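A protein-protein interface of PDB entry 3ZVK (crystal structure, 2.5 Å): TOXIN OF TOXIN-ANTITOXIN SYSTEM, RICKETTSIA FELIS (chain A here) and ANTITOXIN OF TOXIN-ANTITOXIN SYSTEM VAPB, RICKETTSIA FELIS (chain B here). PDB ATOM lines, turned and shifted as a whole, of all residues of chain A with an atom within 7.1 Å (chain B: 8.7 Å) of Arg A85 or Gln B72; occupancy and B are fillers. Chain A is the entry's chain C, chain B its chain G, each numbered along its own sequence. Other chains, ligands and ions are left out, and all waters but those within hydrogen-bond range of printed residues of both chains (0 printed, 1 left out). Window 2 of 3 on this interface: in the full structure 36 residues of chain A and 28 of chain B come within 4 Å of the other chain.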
ATOM      1  N   TYR A  80     -16.942 -16.107  23.603  1.00  0.00           N
ATOM      2  CA  TYR A  80     -17.607 -15.398  22.514  1.00  0.00           C
ATOM      3  C   TYR A  80     -16.887 -15.587  21.205  1.00  0.00           C
ATOM      4  O   TYR A  80     -17.548 -15.845  20.197  1.00  0.00           O
ATOM      5  CB  TYR A  80     -17.802 -13.896  22.852  1.00  0.00           C
ATOM      6  CG  TYR A  80     -18.594 -13.700  24.115  1.00  0.00           C
ATOM      7  CD1 TYR A  80     -19.978 -13.866  24.125  1.00  0.00           C
ATOM      8  CD2 TYR A  80     -17.959 -13.455  25.324  1.00  0.00           C
ATOM      9  CE1 TYR A  80     -20.717 -13.728  25.302  1.00  0.00           C
ATOM     10  CE2 TYR A  80     -18.683 -13.334  26.511  1.00  0.00           C
ATOM     11  CZ  TYR A  80     -20.063 -13.470  26.495  1.00  0.00           C
ATOM     12  OH  TYR A  80     -20.778 -13.330  27.656  1.00  0.00           O
ATOM     13  N   TYR A  81     -15.538 -15.522  21.223  1.00  0.00           N
ATOM     14  CA  TYR A  81     -14.700 -15.769  20.039  1.00  0.00           C
ATOM     15  C   TYR A  81     -14.944 -17.189  19.466  1.00  0.00           C
ATOM     16  O   TYR A  81     -15.092 -17.342  18.255  1.00  0.00           O
ATOM     17  CB  TYR A  81     -13.208 -15.539  20.365  1.00  0.00           C
ATOM     18  CG  TYR A  81     -12.258 -15.983  19.273  1.00  0.00           C
ATOM     19  CD1 TYR A  81     -11.782 -17.296  19.224  1.00  0.00           C
ATOM     20  CD2 TYR A  81     -11.834 -15.099  18.286  1.00  0.00           C
ATOM     21  CE1 TYR A  81     -10.910 -17.721  18.224  1.00  0.00           C
ATOM     22  CE2 TYR A  81     -10.939 -15.505  17.294  1.00  0.00           C
ATOM     23  CZ  TYR A  81     -10.473 -16.820  17.275  1.00  0.00           C
ATOM     24  OH  TYR A  81      -9.625 -17.281  16.288  1.00  0.00           O
ATOM     25  N   GLY A  82     -14.949 -18.199  20.331  1.00  0.00           N
ATOM     26  CA  GLY A  82     -15.163 -19.585  19.935  1.00  0.00           C
ATOM     27  C   GLY A  82     -16.498 -19.821  19.271  1.00  0.00           C
ATOM     28  O   GLY A  82     -16.574 -20.506  18.249  1.00  0.00           O
ATOM     29  N   GLU A  83     -17.553 -19.224  19.831  1.00  0.00           N
ATOM     30  CA  GLU A  83     -18.931 -19.310  19.319  1.00  0.00           C
ATOM     31  C   GLU A  83     -19.108 -18.566  17.988  1.00  0.00           C
ATOM     32  O   GLU A  83     -19.741 -19.095  17.060  1.00  0.00           O
ATOM     33  CB  GLU A  83     -19.938 -18.793  20.370  1.00  0.00           C
ATOM     34  CG  GLU A  83     -20.091 -19.700  21.573  1.00  0.00           C
ATOM     35  CD  GLU A  83     -20.852 -20.985  21.326  1.00  0.00           C
ATOM     36  OE1 GLU A  83     -22.101 -20.940  21.254  1.00  0.00           O
ATOM     37  OE2 GLU A  83     -20.196 -22.045  21.233  1.00  0.00           O
ATOM     38  N   LEU A  84     -18.538 -17.346  17.902  1.00  0.00           N
ATOM     39  CA  LEU A  84     -18.606 -16.484  16.717  1.00  0.00           C
ATOM     40  C   LEU A  84     -17.830 -17.095  15.522  1.00  0.00           C
ATOM     41  O   LEU A  84     -18.364 -17.158  14.414  1.00  0.00           O
ATOM     42  CB  LEU A  84     -18.110 -15.057  17.070  1.00  0.00           C
ATOM     43  CG  LEU A  84     -18.041 -14.030  15.941  1.00  0.00           C
ATOM     44  CD1 LEU A  84     -19.412 -13.834  15.271  1.00  0.00           C
ATOM     45  CD2 LEU A  84     -17.473 -12.708  16.431  1.00  0.00           C
ATOM     46  N   ARG A  85     -16.597 -17.566  15.762  1.00  0.00           N
ATOM     47  CA  ARG A  85     -15.772 -18.175  14.718  1.00  0.00           C
ATOM     48  C   ARG A  85     -16.446 -19.405  14.140  1.00  0.00           C
ATOM     49  O   ARG A  85     -16.489 -19.541  12.923  1.00  0.00           O
ATOM     50  CB  ARG A  85     -14.362 -18.494  15.237  1.00  0.00           C
ATOM     51  CG  ARG A  85     -13.424 -18.920  14.130  1.00  0.00           C
ATOM     52  CD  ARG A  85     -12.016 -19.073  14.594  1.00  0.00           C
ATOM     53  NE  ARG A  85     -11.280 -19.832  13.597  1.00  0.00           N
ATOM     54  CZ  ARG A  85     -10.061 -20.309  13.782  1.00  0.00           C
ATOM     55  NH1 ARG A  85      -9.434 -20.106  14.928  1.00  0.00           N
ATOM     56  NH2 ARG A  85      -9.469 -21.020  12.832  1.00  0.00           N
ATOM     57  N   THR A  86     -17.011 -20.275  14.996  1.00  0.00           N
ATOM     58  CA  THR A  86     -17.726 -21.490  14.572  1.00  0.00           C
ATOM     59  C   THR A  86     -18.934 -21.139  13.694  1.00  0.00           C
ATOM     60  O   THR A  86     -19.100 -21.724  12.620  1.00  0.00           O
ATOM     61  CB  THR A  86     -18.115 -22.330  15.797  1.00  0.00           C
ATOM     62  OG1 THR A  86     -16.918 -22.701  16.480  1.00  0.00           O
ATOM     63  CG2 THR A  86     -18.914 -23.576  15.436  1.00  0.00           C
ATOM     64  N   GLU A  87     -19.757 -20.175  14.146  1.00  0.00           N
ATOM     65  CA  GLU A  87     -20.943 -19.740  13.430  1.00  0.00           C
ATOM     66  C   GLU A  87     -20.604 -19.133  12.058  1.00  0.00           C
ATOM     67  O   GLU A  87     -21.235 -19.499  11.074  1.00  0.00           O
ATOM     68  CB  GLU A  87     -21.762 -18.763  14.291  1.00  0.00           C
ATOM     69  CG  GLU A  87     -23.165 -18.549  13.734  1.00  0.00           C
ATOM     70  CD  GLU A  87     -24.069 -17.562  14.443  1.00  0.00           C
ATOM     71  OE1 GLU A  87     -23.655 -16.994  15.483  1.00  0.00           O
ATOM     72  OE2 GLU A  87     -25.188 -17.331  13.927  1.00  0.00           O
ATOM     73  N   LEU A  88     -19.599 -18.240  11.990  1.00  0.00           N
ATOM     74  CA  LEU A  88     -19.189 -17.602  10.741  1.00  0.00           C
ATOM     75  C   LEU A  88     -18.692 -18.599   9.727  1.00  0.00           C
ATOM     76  O   LEU A  88     -19.035 -18.499   8.540  1.00  0.00           O
ATOM     77  CB  LEU A  88     -18.144 -16.506  10.992  1.00  0.00           C
ATOM     78  CG  LEU A  88     -18.634 -15.273  11.745  1.00  0.00           C
ATOM     79  CD1 LEU A  88     -17.529 -14.313  11.951  1.00  0.00           C
ATOM     80  CD2 LEU A  88     -19.777 -14.588  11.019  1.00  0.00           C
ATOM     81  N   GLU A  89     -17.915 -19.596  10.197  1.00  0.00           N
ATOM     82  CA  GLU A  89     -17.366 -20.647   9.336  1.00  0.00           C
ATOM     83  C   GLU A  89     -18.470 -21.549   8.817  1.00  0.00           C
ATOM     84  O   GLU A  89     -18.474 -21.867   7.635  1.00  0.00           O
ATOM     85  CB  GLU A  89     -16.306 -21.448  10.082  1.00  0.00           C
ATOM     86  CG  GLU A  89     -15.069 -20.636  10.370  1.00  0.00           C
ATOM     87  CD  GLU A  89     -14.010 -21.435  11.074  1.00  0.00           C
ATOM     88  OE1 GLU A  89     -14.300 -22.572  11.523  1.00  0.00           O
ATOM     89  OE2 GLU A  89     -12.863 -20.943  11.110  1.00  0.00           O
ATOM     90  N   GLN A  90     -19.441 -21.893   9.683  1.00  0.00           N
ATOM     91  CA  GLN A  90     -20.613 -22.699   9.340  1.00  0.00           C
ATOM     92  C   GLN A  90     -21.417 -22.052   8.214  1.00  0.00           C
ATOM     93  O   GLN A  90     -21.931 -22.761   7.349  1.00  0.00           O
ATOM     94  CB  GLN A  90     -21.508 -22.858  10.581  1.00  0.00           C
ATOM     95  CG  GLN A  90     -21.658 -24.282  11.068  1.00  0.00           C
ATOM     96  CD  GLN A  90     -21.445 -24.401  12.555  1.00  0.00           C
ATOM     97  OE1 GLN A  90     -22.091 -23.720  13.377  1.00  0.00           O
ATOM     98  NE2 GLN A  90     -20.519 -25.277  12.933  1.00  0.00           N
ATOM     99  N   LYS A  91     -21.538 -20.704   8.229  1.00  0.00           N
ATOM    100  CA  LYS A  91     -22.318 -19.958   7.215  1.00  0.00           C
ATOM    101  C   LYS A  91     -21.470 -19.595   5.972  1.00  0.00           C
ATOM    102  O   LYS A  91     -21.979 -18.962   5.062  1.00  0.00           O
ATOM    103  CB  LYS A  91     -22.947 -18.673   7.815  1.00  0.00           C
ATOM    104  CG  LYS A  91     -23.629 -18.807   9.170  1.00  0.00           C
ATOM    105  CD  LYS A  91     -24.969 -19.576   9.190  1.00  0.00           C
ATOM    106  CE  LYS A  91     -25.637 -19.525  10.566  1.00  0.00           C
ATOM    107  NZ  LYS A  91     -26.174 -18.178  10.915  1.00  0.00           N
ATOM    108  N   LEU A  93     -18.923 -17.458   5.973  1.00  0.00           N
ATOM    109  CA  LEU A  93     -18.637 -16.029   6.080  1.00  0.00           C
ATOM    110  C   LEU A  93     -17.197 -15.778   6.459  1.00  0.00           C
ATOM    111  O   LEU A  93     -16.758 -16.183   7.533  1.00  0.00           O
ATOM    112  CB  LEU A  93     -19.582 -15.346   7.092  1.00  0.00           C
ATOM    113  CG  LEU A  93     -20.966 -14.771   6.686  1.00  0.00           C
ATOM    114  CD1 LEU A  93     -21.465 -15.211   5.318  1.00  0.00           C
ATOM    115  CD2 LEU A  93     -22.023 -15.013   7.777  1.00  0.00           C
ATOM    116  N   ILE A  95     -13.984 -13.598   7.512  1.00  0.00           N
ATOM    117  CA  ILE A  95     -13.575 -12.537   8.433  1.00  0.00           C
ATOM    118  C   ILE A  95     -12.088 -12.732   8.752  1.00  0.00           C
ATOM    119  O   ILE A  95     -11.649 -13.872   8.961  1.00  0.00           O
ATOM    120  CB  ILE A  95     -14.472 -12.457   9.698  1.00  0.00           C
ATOM    121  CG1 ILE A  95     -14.032 -11.329  10.631  1.00  0.00           C
ATOM    122  CG2 ILE A  95     -14.536 -13.809  10.423  1.00  0.00           C
ATOM    123  CD1 ILE A  95     -15.143 -10.671  11.381  1.00  0.00           C
ATOM    124  N   ASN A  97      -8.514 -12.543  10.758  1.00  0.00           N
ATOM    125  CA  ASN A  97      -8.161 -12.970  12.089  1.00  0.00           C
ATOM    126  C   ASN A  97      -8.354 -11.904  13.182  1.00  0.00           C
ATOM    127  O   ASN A  97      -8.898 -12.211  14.244  1.00  0.00           O
ATOM    128  CB  ASN A  97      -6.736 -13.496  12.112  1.00  0.00           C
ATOM    129  CG  ASN A  97      -6.446 -14.212  13.398  1.00  0.00           C
ATOM    130  OD1 ASN A  97      -7.218 -15.059  13.841  1.00  0.00           O
ATOM    131  ND2 ASN A  97      -5.462 -13.733  14.129  1.00  0.00           N
ATOM    132  N   LEU A 100     -12.074 -10.612  13.753  1.00  0.00           N
ATOM    133  CA  LEU A 100     -12.793 -11.647  14.481  1.00  0.00           C
ATOM    134  C   LEU A 100     -12.542 -11.497  15.998  1.00  0.00           C
ATOM    135  O   LEU A 100     -13.485 -11.593  16.788  1.00  0.00           O
ATOM    136  CB  LEU A 100     -12.326 -13.014  13.956  1.00  0.00           C
ATOM    137  CG  LEU A 100     -12.968 -14.283  14.498  1.00  0.00           C
ATOM    138  CD1 LEU A 100     -14.492 -14.252  14.395  1.00  0.00           C
ATOM    139  CD2 LEU A 100     -12.427 -15.465  13.761  1.00  0.00           C
ATOM    140  N   SER A 104     -15.391  -9.994  18.762  1.00  0.00           N
ATOM    141  CA  SER A 104     -15.641 -10.846  19.939  1.00  0.00           C
ATOM    142  C   SER A 104     -15.443 -10.064  21.226  1.00  0.00           C
ATOM    143  O   SER A 104     -16.106 -10.340  22.245  1.00  0.00           O
ATOM    144  CB  SER A 104     -14.654 -12.021  19.957  1.00  0.00           C
ATOM    145  OG  SER A 104     -14.819 -12.821  18.799  1.00  0.00           O
ATOM    146  N   LEU B  69      -5.654 -11.606   7.132  1.00  0.00           N
ATOM    147  CA  LEU B  69      -5.993 -12.890   6.512  1.00  0.00           C
ATOM    148  C   LEU B  69      -6.871 -13.713   7.463  1.00  0.00           C
ATOM    149  O   LEU B  69      -6.797 -13.488   8.669  1.00  0.00           O
ATOM    150  CB  LEU B  69      -4.711 -13.676   6.154  1.00  0.00           C
ATOM    151  CG  LEU B  69      -3.879 -13.196   4.958  1.00  0.00           C
ATOM    152  CD1 LEU B  69      -2.692 -14.120   4.729  1.00  0.00           C
ATOM    153  CD2 LEU B  69      -4.721 -13.101   3.653  1.00  0.00           C
ATOM    154  N   PRO B  70      -7.677 -14.693   6.978  1.00  0.00           N
ATOM    155  CA  PRO B  70      -8.518 -15.505   7.901  1.00  0.00           C
ATOM    156  C   PRO B  70      -7.732 -16.221   9.005  1.00  0.00           C
ATOM    157  O   PRO B  70      -6.542 -16.489   8.799  1.00  0.00           O
ATOM    158  CB  PRO B  70      -9.153 -16.543   6.973  1.00  0.00           C
ATOM    159  CG  PRO B  70      -9.114 -15.922   5.642  1.00  0.00           C
ATOM    160  CD  PRO B  70      -7.871 -15.115   5.579  1.00  0.00           C
ATOM    161  N   PRO B  71      -8.352 -16.577  10.160  1.00  0.00           N
ATOM    162  CA  PRO B  71      -7.579 -17.242  11.233  1.00  0.00           C
ATOM    163  C   PRO B  71      -6.884 -18.510  10.766  1.00  0.00           C
ATOM    164  O   PRO B  71      -7.406 -19.207   9.887  1.00  0.00           O
ATOM    165  CB  PRO B  71      -8.624 -17.547  12.317  1.00  0.00           C
ATOM    166  CG  PRO B  71      -9.943 -17.330  11.684  1.00  0.00           C
ATOM    167  CD  PRO B  71      -9.752 -16.348  10.581  1.00  0.00           C
ATOM    168  N   GLN B  72      -5.691 -18.790  11.319  1.00  0.00           N
ATOM    169  CA  GLN B  72      -4.959 -19.976  10.914  1.00  0.00           C
ATOM    170  C   GLN B  72      -5.694 -21.265  11.305  1.00  0.00           C
ATOM    171  O   GLN B  72      -6.418 -21.305  12.310  1.00  0.00           O
ATOM    172  CB  GLN B  72      -3.515 -19.947  11.413  1.00  0.00           C
ATOM    173  CG  GLN B  72      -3.387 -20.029  12.917  1.00  0.00           C
ATOM    174  CD  GLN B  72      -1.950 -19.967  13.319  1.00  0.00           C
ATOM    175  OE1 GLN B  72      -1.475 -18.929  13.763  1.00  0.00           O
ATOM    176  NE2 GLN B  72      -1.216 -21.057  13.128  1.00  0.00           N
ATOM    177  N   LYS B  73      -5.544 -22.297  10.470  1.00  0.00           N
ATOM    178  CA  LYS B  73      -6.211 -23.567  10.735  1.00  0.00           C
ATOM    179  C   LYS B  73      -5.340 -24.491  11.574  1.00  0.00           C
ATOM    180  O   LYS B  73      -4.094 -24.402  11.540  1.00  0.00           O
ATOM    181  CB  LYS B  73      -6.698 -24.254   9.435  1.00  0.00           C
ATOM    182  CG  LYS B  73      -7.779 -23.468   8.697  1.00  0.00           C
ATOM    183  CD  LYS B  73      -8.137 -24.098   7.344  1.00  0.00           C
ATOM    184  CE  LYS B  73      -8.809 -23.087   6.461  1.00  0.00           C
ATOM    185  NZ  LYS B  73      -7.813 -22.194   5.787  1.00  0.00           N
ATOM    186  N   ARG B  74      -6.017 -25.318  12.394  1.00  0.00           N
ATOM    187  CA  ARG B  74      -5.402 -26.330  13.260  1.00  0.00           C
ATOM    188  C   ARG B  74      -6.334 -27.525  13.370  1.00  0.00           C
ATOM    189  O   ARG B  74      -7.544 -27.399  13.157  1.00  0.00           O
ATOM    190  CB  ARG B  74      -5.146 -25.819  14.686  1.00  0.00           C
ATOM    191  CG  ARG B  74      -4.319 -24.565  14.829  1.00  0.00           C
ATOM    192  CD  ARG B  74      -3.977 -24.325  16.289  1.00  0.00           C
ATOM    193  NE  ARG B  74      -3.473 -22.972  16.509  1.00  0.00           N
ATOM    194  CZ  ARG B  74      -2.205 -22.588  16.375  1.00  0.00           C
ATOM    195  NH1 ARG B  74      -1.272 -23.463  16.024  1.00  0.00           N
ATOM    196  NH2 ARG B  74      -1.863 -21.327  16.592  1.00  0.00           N
ATOM    197  N   LYS B  75      -5.767 -28.683  13.711  1.00  0.00           N
ATOM    198  CA  LYS B  75      -6.509 -29.872  14.080  1.00  0.00           C
ATOM    199  C   LYS B  75      -6.938 -29.519  15.507  1.00  0.00           C
ATOM    200  O   LYS B  75      -6.188 -28.876  16.270  1.00  0.00           O
ATOM    201  CB  LYS B  75      -5.538 -31.059  14.123  1.00  0.00           C
ATOM    202  CG  LYS B  75      -6.125 -32.425  14.496  1.00  0.00           C
ATOM    203  CD  LYS B  75      -4.989 -33.399  14.727  1.00  0.00           C
ATOM    204  CE  LYS B  75      -5.425 -34.831  14.927  1.00  0.00           C
ATOM    205  NZ  LYS B  75      -4.256 -35.769  14.941  1.00  0.00           N
ATOM    206  N   TYR B  76      -8.150 -29.850  15.869  1.00  0.00           N
ATOM    207  CA  TYR B  76      -8.541 -29.523  17.251  1.00  0.00           C
ATOM    208  C   TYR B  76      -8.917 -30.818  17.929  1.00  0.00           C
ATOM    209  O   TYR B  76      -8.069 -31.711  17.977  1.00  0.00           O
ATOM    210  CB  TYR B  76      -9.591 -28.402  17.324  1.00  0.00           C
ATOM    211  CG  TYR B  76      -8.987 -27.014  17.176  1.00  0.00           C
ATOM    212  CD1 TYR B  76      -8.480 -26.330  18.282  1.00  0.00           C
ATOM    213  CD2 TYR B  76      -8.912 -26.387  15.931  1.00  0.00           C
ATOM    214  CE1 TYR B  76      -7.892 -25.076  18.145  1.00  0.00           C
ATOM    215  CE2 TYR B  76      -8.347 -25.120  15.793  1.00  0.00           C
ATOM    216  CZ  TYR B  76      -7.802 -24.489  16.897  1.00  0.00           C
ATOM    217  OH  TYR B  76      -7.187 -23.265  16.774  1.00  0.00           O
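The guanidinium group (NH2) of Arg A85 sits at hydrogen-bond distance from the backbone carbonyl oxygen (O) of Gln B72, at 3.1 Å. The backbone NH (N) of Asn A97 is in hydrogen-bond range of the backbone carbonyl oxygen (O) of Leu B69, at 2.9 Å.
The guanidinium group (NH1) of Arg A85 is in hydrogen-bond range of the side-chain hydroxyl (OH) of Tyr A81 (3.1 Å). OE2 of Glu A89 lies within salt-bridge range of NE of Arg A85, 3.2 Å away. The backbone carbonyl oxygen (O) of Leu A100 sits at hydrogen-bond distance from the side-chain hydroxyl (OG) of Ser A104, 2.7 Å away.
Among the printed residues, pairs that only touch across the chains: Asn A97 with Pro B71, Arg A85 with Pro B71, Ile A95 with Pro B71, Ile A95 with Pro B70 and Leu A100 with Pro B71.
Of chain B, only Pro B71 and Gln B72 come within 4 Å of Arg A85. Lys A91 touches none of the printed residues of chain B. Leu A93 touches none of the printed residues of chain B. Printed residues of chain B within 4 Å of Ile A95: Pro B70 (3.7 Å) and Pro B71 (3.5 Å). Printed residues of chain B within 4 Å of Asn A97: Leu B69 and Pro B71. Printed residues of chain B within 4 Å of Leu A100: Pro B71. Of the printed residues of chain A, Leu B69 touches Asn A97. Gln B72 touches just one residue of chain A: Arg A85 (3.1 Å). The nearest residue of chain B that does not touch Arg A85 is Tyr B76 (4.3 Å).
Printed residues of chain A that touch a printed residue of chain B: Arg A85, Ile A95, Asn A97 and Leu A100. Hydrophobic or aromatic side chains of chain A that line the printed part of chain B: Leu A100. Printed residues of chain B that touch a printed residue of chain A: Leu B69, Pro B70, Pro B71 and Gln B72. Hydrophobic or aromatic side chains of chain B that line the printed part of chain A: Pro B71. Among the printed residues, 7 pairs touch across the chains. Among the printed residues, no Asp or Glu carboxylate lies within 4 Å of a Lys or Arg side-chain nitrogen of the other chain.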
